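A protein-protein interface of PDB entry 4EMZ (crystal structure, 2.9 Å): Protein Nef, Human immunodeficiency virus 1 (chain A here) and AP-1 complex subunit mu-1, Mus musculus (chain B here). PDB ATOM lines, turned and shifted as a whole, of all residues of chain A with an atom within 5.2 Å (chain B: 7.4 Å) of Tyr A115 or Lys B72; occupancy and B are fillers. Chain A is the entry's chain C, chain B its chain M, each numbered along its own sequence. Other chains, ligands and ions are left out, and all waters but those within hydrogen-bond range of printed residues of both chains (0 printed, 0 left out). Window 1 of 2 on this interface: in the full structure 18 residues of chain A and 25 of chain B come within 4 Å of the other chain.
The side-chain hydroxyl (OG) of Ser B71 is in hydrogen-bond range of the backbone carbonyl oxygen (O) of Pro A122 (3.5 Å).
OD1 of Asn B58 sits at hydrogen-bond distance from N of Gln B234, 2.8 Å away.
Lys B72 touches Tyr A115 (NZ to CE2, 3.7 Å).
Phe A121 touches Gln B234 (CD2 to OE1, 3.3 Å).
Phe A121 touches Arg B236 (CE1 to CA, 3.5 Å).
Lys B72 touches Pro A122.
Of chain B, only Lys B72 comes within 4 Å of Tyr A115.
Lys B72 touches just these residues of chain A: Tyr A115 (3.7 Å) and Pro A122 (3.7 Å).
Of the printed residues of chain A, Gln B234 touches Phe A121 (3.3 Å).
Printed residues of chain B within 4 Å of Pro A122: Ser B71 and Lys B72.
The nearest residue of chain B that does not touch Tyr A115 is Gln B234 (5.2 Å).
The nearest printed residue of chain A that does not touch Lys B72 is Leu A112 (5.2 Å).
Of the 14 printed residues of chain A, 3 touch a printed residue of chain B.
Among the printed residues, 5 pairs touch across the chains.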
ATOM      1  N   LEU A  76       2.115  17.249  19.680  1.00  0.00           N
ATOM      2  CA  LEU A  76       1.499  18.198  20.556  1.00  0.00           C
ATOM      3  C   LEU A  76       0.031  17.878  20.544  1.00  0.00           C
ATOM      4  O   LEU A  76      -0.583  17.767  19.487  1.00  0.00           O
ATOM      5  CB  LEU A  76       1.728  19.610  20.047  1.00  0.00           C
ATOM      6  CG  LEU A  76       3.183  19.992  19.789  1.00  0.00           C
ATOM      7  CD1 LEU A  76       3.291  21.436  19.388  1.00  0.00           C
ATOM      8  CD2 LEU A  76       4.021  19.759  21.008  1.00  0.00           C
ATOM      9  N   LEU A 110       3.441  27.599  34.868  1.00  0.00           N
ATOM     10  CA  LEU A 110       3.016  26.185  34.929  1.00  0.00           C
ATOM     11  C   LEU A 110       2.764  25.643  33.517  1.00  0.00           C
ATOM     12  O   LEU A 110       3.332  24.642  33.064  1.00  0.00           O
ATOM     13  CB  LEU A 110       1.730  26.020  35.739  1.00  0.00           C
ATOM     14  CG  LEU A 110       1.664  24.844  36.709  1.00  0.00           C
ATOM     15  CD1 LEU A 110       0.345  24.863  37.469  1.00  0.00           C
ATOM     16  CD2 LEU A 110       1.855  23.492  36.056  1.00  0.00           C
ATOM     17  N   ASP A 111       1.887  26.346  32.814  1.00  0.00           N
ATOM     18  CA  ASP A 111       1.442  25.895  31.509  1.00  0.00           C
ATOM     19  C   ASP A 111       2.604  25.694  30.545  1.00  0.00           C
ATOM     20  O   ASP A 111       2.732  24.637  29.920  1.00  0.00           O
ATOM     21  CB  ASP A 111       0.449  26.885  30.943  1.00  0.00           C
ATOM     22  CG  ASP A 111      -0.754  27.083  31.858  1.00  0.00           C
ATOM     23  OD1 ASP A 111      -1.234  26.093  32.422  1.00  0.00           O
ATOM     24  OD2 ASP A 111      -1.187  28.245  32.047  1.00  0.00           O
ATOM     25  N   LEU A 112       3.474  26.692  30.437  1.00  0.00           N
ATOM     26  CA  LEU A 112       4.643  26.559  29.571  1.00  0.00           C
ATOM     27  C   LEU A 112       5.468  25.390  30.000  1.00  0.00           C
ATOM     28  O   LEU A 112       5.956  24.642  29.167  1.00  0.00           O
ATOM     29  CB  LEU A 112       5.514  27.799  29.584  1.00  0.00           C
ATOM     30  CG  LEU A 112       5.096  28.762  28.468  1.00  0.00           C
ATOM     31  CD1 LEU A 112       3.579  28.996  28.441  1.00  0.00           C
ATOM     32  CD2 LEU A 112       5.852  30.074  28.570  1.00  0.00           C
ATOM     33  N   TRP A 113       5.600  25.205  31.301  1.00  0.00           N
ATOM     34  CA  TRP A 113       6.402  24.091  31.755  1.00  0.00           C
ATOM     35  C   TRP A 113       5.879  22.789  31.178  1.00  0.00           C
ATOM     36  O   TRP A 113       6.632  21.971  30.614  1.00  0.00           O
ATOM     37  CB  TRP A 113       6.499  24.081  33.278  1.00  0.00           C
ATOM     38  CG  TRP A 113       7.193  22.883  33.812  1.00  0.00           C
ATOM     39  CD1 TRP A 113       8.457  22.390  33.473  1.00  0.00           C
ATOM     40  CD2 TRP A 113       6.646  21.950  34.759  1.00  0.00           C
ATOM     41  NE1 TRP A 113       8.722  21.251  34.164  1.00  0.00           N
ATOM     42  CE2 TRP A 113       7.667  20.931  34.957  1.00  0.00           C
ATOM     43  CE3 TRP A 113       5.475  21.881  35.479  1.00  0.00           C
ATOM     44  CZ2 TRP A 113       7.486  19.893  35.830  1.00  0.00           C
ATOM     45  CZ3 TRP A 113       5.293  20.816  36.340  1.00  0.00           C
ATOM     46  CH2 TRP A 113       6.276  19.845  36.516  1.00  0.00           C
ATOM     47  N   ILE A 114       4.563  22.602  31.296  1.00  0.00           N
ATOM     48  CA  ILE A 114       3.910  21.366  30.818  1.00  0.00           C
ATOM     49  C   ILE A 114       3.953  21.276  29.279  1.00  0.00           C
ATOM     50  O   ILE A 114       4.227  20.227  28.711  1.00  0.00           O
ATOM     51  CB  ILE A 114       2.454  21.296  31.337  1.00  0.00           C
ATOM     52  CG1 ILE A 114       2.450  21.123  32.852  1.00  0.00           C
ATOM     53  CG2 ILE A 114       1.623  20.207  30.636  1.00  0.00           C
ATOM     54  CD1 ILE A 114       3.220  19.909  33.303  1.00  0.00           C
ATOM     55  N   TYR A 115       3.699  22.394  28.620  1.00  0.00           N
ATOM     56  CA  TYR A 115       3.867  22.486  27.186  1.00  0.00           C
ATOM     57  C   TYR A 115       5.269  22.048  26.733  1.00  0.00           C
ATOM     58  O   TYR A 115       5.402  21.268  25.799  1.00  0.00           O
ATOM     59  CB  TYR A 115       3.566  23.912  26.724  1.00  0.00           C
ATOM     60  CG  TYR A 115       3.550  24.103  25.227  1.00  0.00           C
ATOM     61  CD1 TYR A 115       3.274  23.059  24.355  1.00  0.00           C
ATOM     62  CD2 TYR A 115       3.791  25.356  24.689  1.00  0.00           C
ATOM     63  CE1 TYR A 115       3.286  23.278  22.995  1.00  0.00           C
ATOM     64  CE2 TYR A 115       3.780  25.572  23.342  1.00  0.00           C
ATOM     65  CZ  TYR A 115       3.543  24.534  22.509  1.00  0.00           C
ATOM     66  OH  TYR A 115       3.557  24.790  21.177  1.00  0.00           O
ATOM     67  N   HIS A 116       6.317  22.529  27.399  1.00  0.00           N
ATOM     68  CA  HIS A 116       7.680  22.246  26.923  1.00  0.00           C
ATOM     69  C   HIS A 116       8.118  20.852  27.302  1.00  0.00           C
ATOM     70  O   HIS A 116       8.714  20.150  26.506  1.00  0.00           O
ATOM     71  CB  HIS A 116       8.682  23.321  27.368  1.00  0.00           C
ATOM     72  CG  HIS A 116       8.327  24.713  26.891  1.00  0.00           C
ATOM     73  ND1 HIS A 116       8.184  25.020  25.585  1.00  0.00           N
ATOM     74  CD2 HIS A 116       8.045  25.882  27.599  1.00  0.00           C
ATOM     75  CE1 HIS A 116       7.850  26.319  25.460  1.00  0.00           C
ATOM     76  NE2 HIS A 116       7.770  26.849  26.689  1.00  0.00           N
ATOM     77  N   THR A 117       7.798  20.406  28.502  1.00  0.00           N
ATOM     78  CA  THR A 117       8.260  19.078  28.935  1.00  0.00           C
ATOM     79  C   THR A 117       7.369  17.909  28.490  1.00  0.00           C
ATOM     80  O   THR A 117       7.863  16.862  28.095  1.00  0.00           O
ATOM     81  CB  THR A 117       8.364  19.022  30.452  1.00  0.00           C
ATOM     82  OG1 THR A 117       7.085  19.274  31.040  1.00  0.00           O
ATOM     83  CG2 THR A 117       9.342  20.065  30.945  1.00  0.00           C
ATOM     84  N   GLN A 118       6.058  18.097  28.564  1.00  0.00           N
ATOM     85  CA  GLN A 118       5.074  17.059  28.235  1.00  0.00           C
ATOM     86  C   GLN A 118       4.270  17.314  26.959  1.00  0.00           C
ATOM     87  O   GLN A 118       3.384  16.547  26.593  1.00  0.00           O
ATOM     88  CB  GLN A 118       4.063  16.938  29.366  1.00  0.00           C
ATOM     89  CG  GLN A 118       4.554  16.337  30.661  1.00  0.00           C
ATOM     90  CD  GLN A 118       3.408  15.676  31.387  1.00  0.00           C
ATOM     91  OE1 GLN A 118       2.785  16.305  32.233  1.00  0.00           O
ATOM     92  NE2 GLN A 118       3.060  14.424  31.000  1.00  0.00           N
ATOM     93  N   GLY A 119       4.491  18.437  26.325  1.00  0.00           N
ATOM     94  CA  GLY A 119       3.873  18.700  25.028  1.00  0.00           C
ATOM     95  C   GLY A 119       2.352  18.859  24.975  1.00  0.00           C
ATOM     96  O   GLY A 119       1.729  18.440  23.995  1.00  0.00           O
ATOM     97  N   TYR A 120       1.745  19.444  26.016  1.00  0.00           N
ATOM     98  CA  TYR A 120       0.295  19.766  25.999  1.00  0.00           C
ATOM     99  C   TYR A 120       0.067  21.230  25.806  1.00  0.00           C
ATOM    100  O   TYR A 120       0.438  22.077  26.637  1.00  0.00           O
ATOM    101  CB  TYR A 120      -0.451  19.367  27.277  1.00  0.00           C
ATOM    102  CG  TYR A 120      -0.401  17.894  27.592  1.00  0.00           C
ATOM    103  CD1 TYR A 120      -1.052  16.967  26.782  1.00  0.00           C
ATOM    104  CD2 TYR A 120       0.343  17.426  28.676  1.00  0.00           C
ATOM    105  CE1 TYR A 120      -0.985  15.616  27.052  1.00  0.00           C
ATOM    106  CE2 TYR A 120       0.433  16.083  28.949  1.00  0.00           C
ATOM    107  CZ  TYR A 120      -0.248  15.187  28.139  1.00  0.00           C
ATOM    108  OH  TYR A 120      -0.164  13.852  28.419  1.00  0.00           O
ATOM    109  N   PHE A 121      -0.614  21.531  24.717  1.00  0.00           N
ATOM    110  CA  PHE A 121      -0.972  22.917  24.404  1.00  0.00           C
ATOM    111  C   PHE A 121      -1.455  23.642  25.661  1.00  0.00           C
ATOM    112  O   PHE A 121      -2.247  23.092  26.431  1.00  0.00           O
ATOM    113  CB  PHE A 121      -2.087  22.951  23.389  1.00  0.00           C
ATOM    114  CG  PHE A 121      -1.713  22.405  22.073  1.00  0.00           C
ATOM    115  CD1 PHE A 121      -2.478  21.445  21.498  1.00  0.00           C
ATOM    116  CD2 PHE A 121      -0.611  22.888  21.375  1.00  0.00           C
ATOM    117  CE1 PHE A 121      -2.160  20.939  20.253  1.00  0.00           C
ATOM    118  CE2 PHE A 121      -0.274  22.384  20.119  1.00  0.00           C
ATOM    119  CZ  PHE A 121      -1.058  21.404  19.563  1.00  0.00           C
ATOM    120  N   PRO A 122      -0.991  24.865  25.881  1.00  0.00           N
ATOM    121  CA  PRO A 122      -1.418  25.578  27.096  1.00  0.00           C
ATOM    122  C   PRO A 122      -2.762  26.313  26.996  1.00  0.00           C
ATOM    123  O   PRO A 122      -2.841  27.488  27.360  1.00  0.00           O
ATOM    124  CB  PRO A 122      -0.315  26.599  27.320  1.00  0.00           C
ATOM    125  CG  PRO A 122       0.270  26.821  25.974  1.00  0.00           C
ATOM    126  CD  PRO A 122       0.014  25.613  25.113  1.00  0.00           C
ATOM    127  N   ASN B  58      -6.578  26.688  17.088  1.00  0.00           N
ATOM    128  CA  ASN B  58      -6.609  27.503  18.279  1.00  0.00           C
ATOM    129  C   ASN B  58      -7.092  28.837  17.856  1.00  0.00           C
ATOM    130  O   ASN B  58      -6.318  29.738  17.607  1.00  0.00           O
ATOM    131  CB  ASN B  58      -5.239  27.584  18.954  1.00  0.00           C
ATOM    132  CG  ASN B  58      -4.199  28.261  18.091  1.00  0.00           C
ATOM    133  OD1 ASN B  58      -4.151  28.057  16.855  1.00  0.00           O
ATOM    134  ND2 ASN B  58      -3.341  29.056  18.717  1.00  0.00           N
ATOM    135  N   ASP B  59      -8.398  28.963  17.833  1.00  0.00           N
ATOM    136  CA  ASP B  59      -9.107  29.957  17.044  1.00  0.00           C
ATOM    137  C   ASP B  59      -9.752  30.922  18.021  1.00  0.00           C
ATOM    138  O   ASP B  59     -10.565  30.550  18.841  1.00  0.00           O
ATOM    139  CB  ASP B  59     -10.079  29.172  16.174  1.00  0.00           C
ATOM    140  CG  ASP B  59     -11.318  29.948  15.731  1.00  0.00           C
ATOM    141  OD1 ASP B  59     -11.354  31.205  15.753  1.00  0.00           O
ATOM    142  OD2 ASP B  59     -12.260  29.222  15.299  1.00  0.00           O
ATOM    143  N   LYS B  60      -9.313  32.169  17.946  1.00  0.00           N
ATOM    144  CA  LYS B  60      -9.567  33.157  19.015  1.00  0.00           C
ATOM    145  C   LYS B  60     -11.033  33.125  19.432  1.00  0.00           C
ATOM    146  O   LYS B  60     -11.377  33.090  20.620  1.00  0.00           O
ATOM    147  CB  LYS B  60      -9.208  34.582  18.563  1.00  0.00           C
ATOM    148  CG  LYS B  60      -9.793  35.633  19.512  1.00  0.00           C
ATOM    149  CD  LYS B  60      -9.065  36.961  19.491  1.00  0.00           C
ATOM    150  CE  LYS B  60      -9.728  37.923  20.465  1.00  0.00           C
ATOM    151  NZ  LYS B  60      -9.356  39.352  20.268  1.00  0.00           N
ATOM    152  N   PHE B  63     -12.112  29.994  21.182  1.00  0.00           N
ATOM    153  CA  PHE B  63     -11.681  30.083  22.574  1.00  0.00           C
ATOM    154  C   PHE B  63     -12.532  31.073  23.364  1.00  0.00           C
ATOM    155  O   PHE B  63     -12.943  30.796  24.487  1.00  0.00           O
ATOM    156  CB  PHE B  63     -10.190  30.449  22.664  1.00  0.00           C
ATOM    157  CG  PHE B  63      -9.257  29.293  22.440  1.00  0.00           C
ATOM    158  CD1 PHE B  63      -9.736  28.087  21.944  1.00  0.00           C
ATOM    159  CD2 PHE B  63      -7.908  29.416  22.725  1.00  0.00           C
ATOM    160  CE1 PHE B  63      -8.893  27.020  21.739  1.00  0.00           C
ATOM    161  CE2 PHE B  63      -7.055  28.357  22.522  1.00  0.00           C
ATOM    162  CZ  PHE B  63      -7.538  27.163  22.008  1.00  0.00           C
ATOM    163  N   ARG B  68     -12.264  29.701  27.216  1.00  0.00           N
ATOM    164  CA  ARG B  68     -10.827  29.554  27.039  1.00  0.00           C
ATOM    165  C   ARG B  68     -10.180  30.820  26.460  1.00  0.00           C
ATOM    166  O   ARG B  68      -8.997  30.807  26.058  1.00  0.00           O
ATOM    167  CB  ARG B  68     -10.561  28.369  26.123  1.00  0.00           C
ATOM    168  CG  ARG B  68     -10.907  27.044  26.776  1.00  0.00           C
ATOM    169  CD  ARG B  68     -10.685  25.872  25.834  1.00  0.00           C
ATOM    170  NE  ARG B  68     -11.446  25.967  24.594  1.00  0.00           N
ATOM    171  CZ  ARG B  68     -11.573  24.976  23.734  1.00  0.00           C
ATOM    172  NH1 ARG B  68     -10.993  23.807  23.961  1.00  0.00           N
ATOM    173  NH2 ARG B  68     -12.303  25.143  22.645  1.00  0.00           N
ATOM    174  N   GLY B  69     -10.952  31.908  26.418  1.00  0.00           N
ATOM    175  CA  GLY B  69     -10.494  33.177  25.831  1.00  0.00           C
ATOM    176  C   GLY B  69      -9.141  33.662  26.330  1.00  0.00           C
ATOM    177  O   GLY B  69      -8.370  34.240  25.565  1.00  0.00           O
ATOM    178  N   LYS B  70      -8.825  33.391  27.594  1.00  0.00           N
ATOM    179  CA  LYS B  70      -7.636  33.962  28.242  1.00  0.00           C
ATOM    180  C   LYS B  70      -6.356  33.312  27.786  1.00  0.00           C
ATOM    181  O   LYS B  70      -5.254  33.659  28.237  1.00  0.00           O
ATOM    182  CB  LYS B  70      -7.721  33.807  29.766  1.00  0.00           C
ATOM    183  CG  LYS B  70      -7.078  34.951  30.556  1.00  0.00           C
ATOM    184  CD  LYS B  70      -7.947  36.226  30.654  1.00  0.00           C
ATOM    185  CE  LYS B  70      -8.674  36.319  32.002  1.00  0.00           C
ATOM    186  NZ  LYS B  70      -9.454  35.099  32.387  1.00  0.00           N
ATOM    187  N   SER B  71      -6.533  32.314  26.919  1.00  0.00           N
ATOM    188  CA  SER B  71      -5.444  31.587  26.300  1.00  0.00           C
ATOM    189  C   SER B  71      -4.922  32.260  25.042  1.00  0.00           C
ATOM    190  O   SER B  71      -5.630  33.053  24.437  1.00  0.00           O
ATOM    191  CB  SER B  71      -5.895  30.162  25.967  1.00  0.00           C
ATOM    192  OG  SER B  71      -5.768  29.351  27.120  1.00  0.00           O
ATOM    193  N   LYS B  72      -3.687  31.924  24.648  1.00  0.00           N
ATOM    194  CA  LYS B  72      -3.076  32.399  23.385  1.00  0.00           C
ATOM    195  C   LYS B  72      -3.741  31.738  22.188  1.00  0.00           C
ATOM    196  O   LYS B  72      -3.864  30.522  22.103  1.00  0.00           O
ATOM    197  CB  LYS B  72      -1.535  32.191  23.337  1.00  0.00           C
ATOM    198  CG  LYS B  72      -1.026  30.740  23.108  1.00  0.00           C
ATOM    199  CD  LYS B  72       0.367  30.383  23.734  1.00  0.00           C
ATOM    200  CE  LYS B  72       1.006  29.095  23.184  1.00  0.00           C
ATOM    201  NZ  LYS B  72       2.512  29.031  23.375  1.00  0.00           N
ATOM    202  N   SER B  73      -4.166  32.566  21.250  1.00  0.00           N
ATOM    203  CA  SER B  73      -4.896  32.088  20.112  1.00  0.00           C
ATOM    204  C   SER B  73      -4.452  32.795  18.840  1.00  0.00           C
ATOM    205  O   SER B  73      -3.471  33.522  18.798  1.00  0.00           O
ATOM    206  CB  SER B  73      -6.383  32.350  20.327  1.00  0.00           C
ATOM    207  OG  SER B  73      -6.635  33.734  20.538  1.00  0.00           O
ATOM    208  N   VAL B  74      -5.208  32.528  17.803  1.00  0.00           N
ATOM    209  CA  VAL B  74      -5.043  33.122  16.525  1.00  0.00           C
ATOM    210  C   VAL B  74      -6.389  33.713  16.126  1.00  0.00           C
ATOM    211  O   VAL B  74      -7.392  33.002  15.991  1.00  0.00           O
ATOM    212  CB  VAL B  74      -4.598  32.015  15.549  1.00  0.00           C
ATOM    213  CG1 VAL B  74      -5.372  31.978  14.220  1.00  0.00           C
ATOM    214  CG2 VAL B  74      -3.113  32.120  15.306  1.00  0.00           C
ATOM    215  N   ARG B 147      16.552  29.214  17.258  1.00  0.00           N
ATOM    216  CA  ARG B 147      16.561  27.775  17.165  1.00  0.00           C
ATOM    217  C   ARG B 147      15.860  27.264  15.920  1.00  0.00           C
ATOM    218  O   ARG B 147      15.774  26.062  15.705  1.00  0.00           O
ATOM    219  CB  ARG B 147      15.944  27.188  18.408  1.00  0.00           C
ATOM    220  CG  ARG B 147      14.448  27.349  18.471  1.00  0.00           C
ATOM    221  CD  ARG B 147      14.035  26.356  19.517  1.00  0.00           C
ATOM    222  NE  ARG B 147      12.604  26.156  19.699  1.00  0.00           N
ATOM    223  CZ  ARG B 147      11.963  24.989  19.551  1.00  0.00           C
ATOM    224  NH1 ARG B 147      12.601  23.888  19.169  1.00  0.00           N
ATOM    225  NH2 ARG B 147      10.659  24.916  19.789  1.00  0.00           N
ATOM    226  N   GLY B 232       1.457  31.589  15.175  1.00  0.00           N
ATOM    227  CA  GLY B 232       1.181  30.829  16.431  1.00  0.00           C
ATOM    228  C   GLY B 232       0.060  29.780  16.326  1.00  0.00           C
ATOM    229  O   GLY B 232      -0.333  29.135  17.318  1.00  0.00           O
ATOM    230  N   GLN B 234      -1.936  26.666  15.908  1.00  0.00           N
ATOM    231  CA  GLN B 234      -1.757  25.298  16.368  1.00  0.00           C
ATOM    232  C   GLN B 234      -2.909  24.589  15.700  1.00  0.00           C
ATOM    233  O   GLN B 234      -4.027  25.126  15.657  1.00  0.00           O
ATOM    234  CB  GLN B 234      -1.954  25.146  17.899  1.00  0.00           C
ATOM    235  CG  GLN B 234      -1.030  25.966  18.807  1.00  0.00           C
ATOM    236  CD  GLN B 234      -1.596  26.158  20.239  1.00  0.00           C
ATOM    237  OE1 GLN B 234      -2.522  25.455  20.657  1.00  0.00           O
ATOM    238  NE2 GLN B 234      -1.041  27.124  20.993  1.00  0.00           N
ATOM    239  N   ARG B 236      -4.863  21.708  16.844  1.00  0.00           N
ATOM    240  CA  ARG B 236      -4.957  21.118  18.191  1.00  0.00           C
ATOM    241  C   ARG B 236      -5.331  19.670  18.107  1.00  0.00           C
ATOM    242  O   ARG B 236      -4.744  18.811  18.773  1.00  0.00           O
ATOM    243  CB  ARG B 236      -5.966  21.892  19.048  1.00  0.00           C
ATOM    244  CG  ARG B 236      -5.530  23.331  19.337  1.00  0.00           C
ATOM    245  CD  ARG B 236      -6.540  24.117  20.137  1.00  0.00           C
ATOM    246  NE  ARG B 236      -6.552  23.633  21.516  1.00  0.00           N
ATOM    247  CZ  ARG B 236      -7.391  22.724  22.005  1.00  0.00           C
ATOM    248  NH1 ARG B 236      -8.342  22.190  21.263  1.00  0.00           N
ATOM    249  NH2 ARG B 236      -7.311  22.359  23.261  1.00  0.00           N
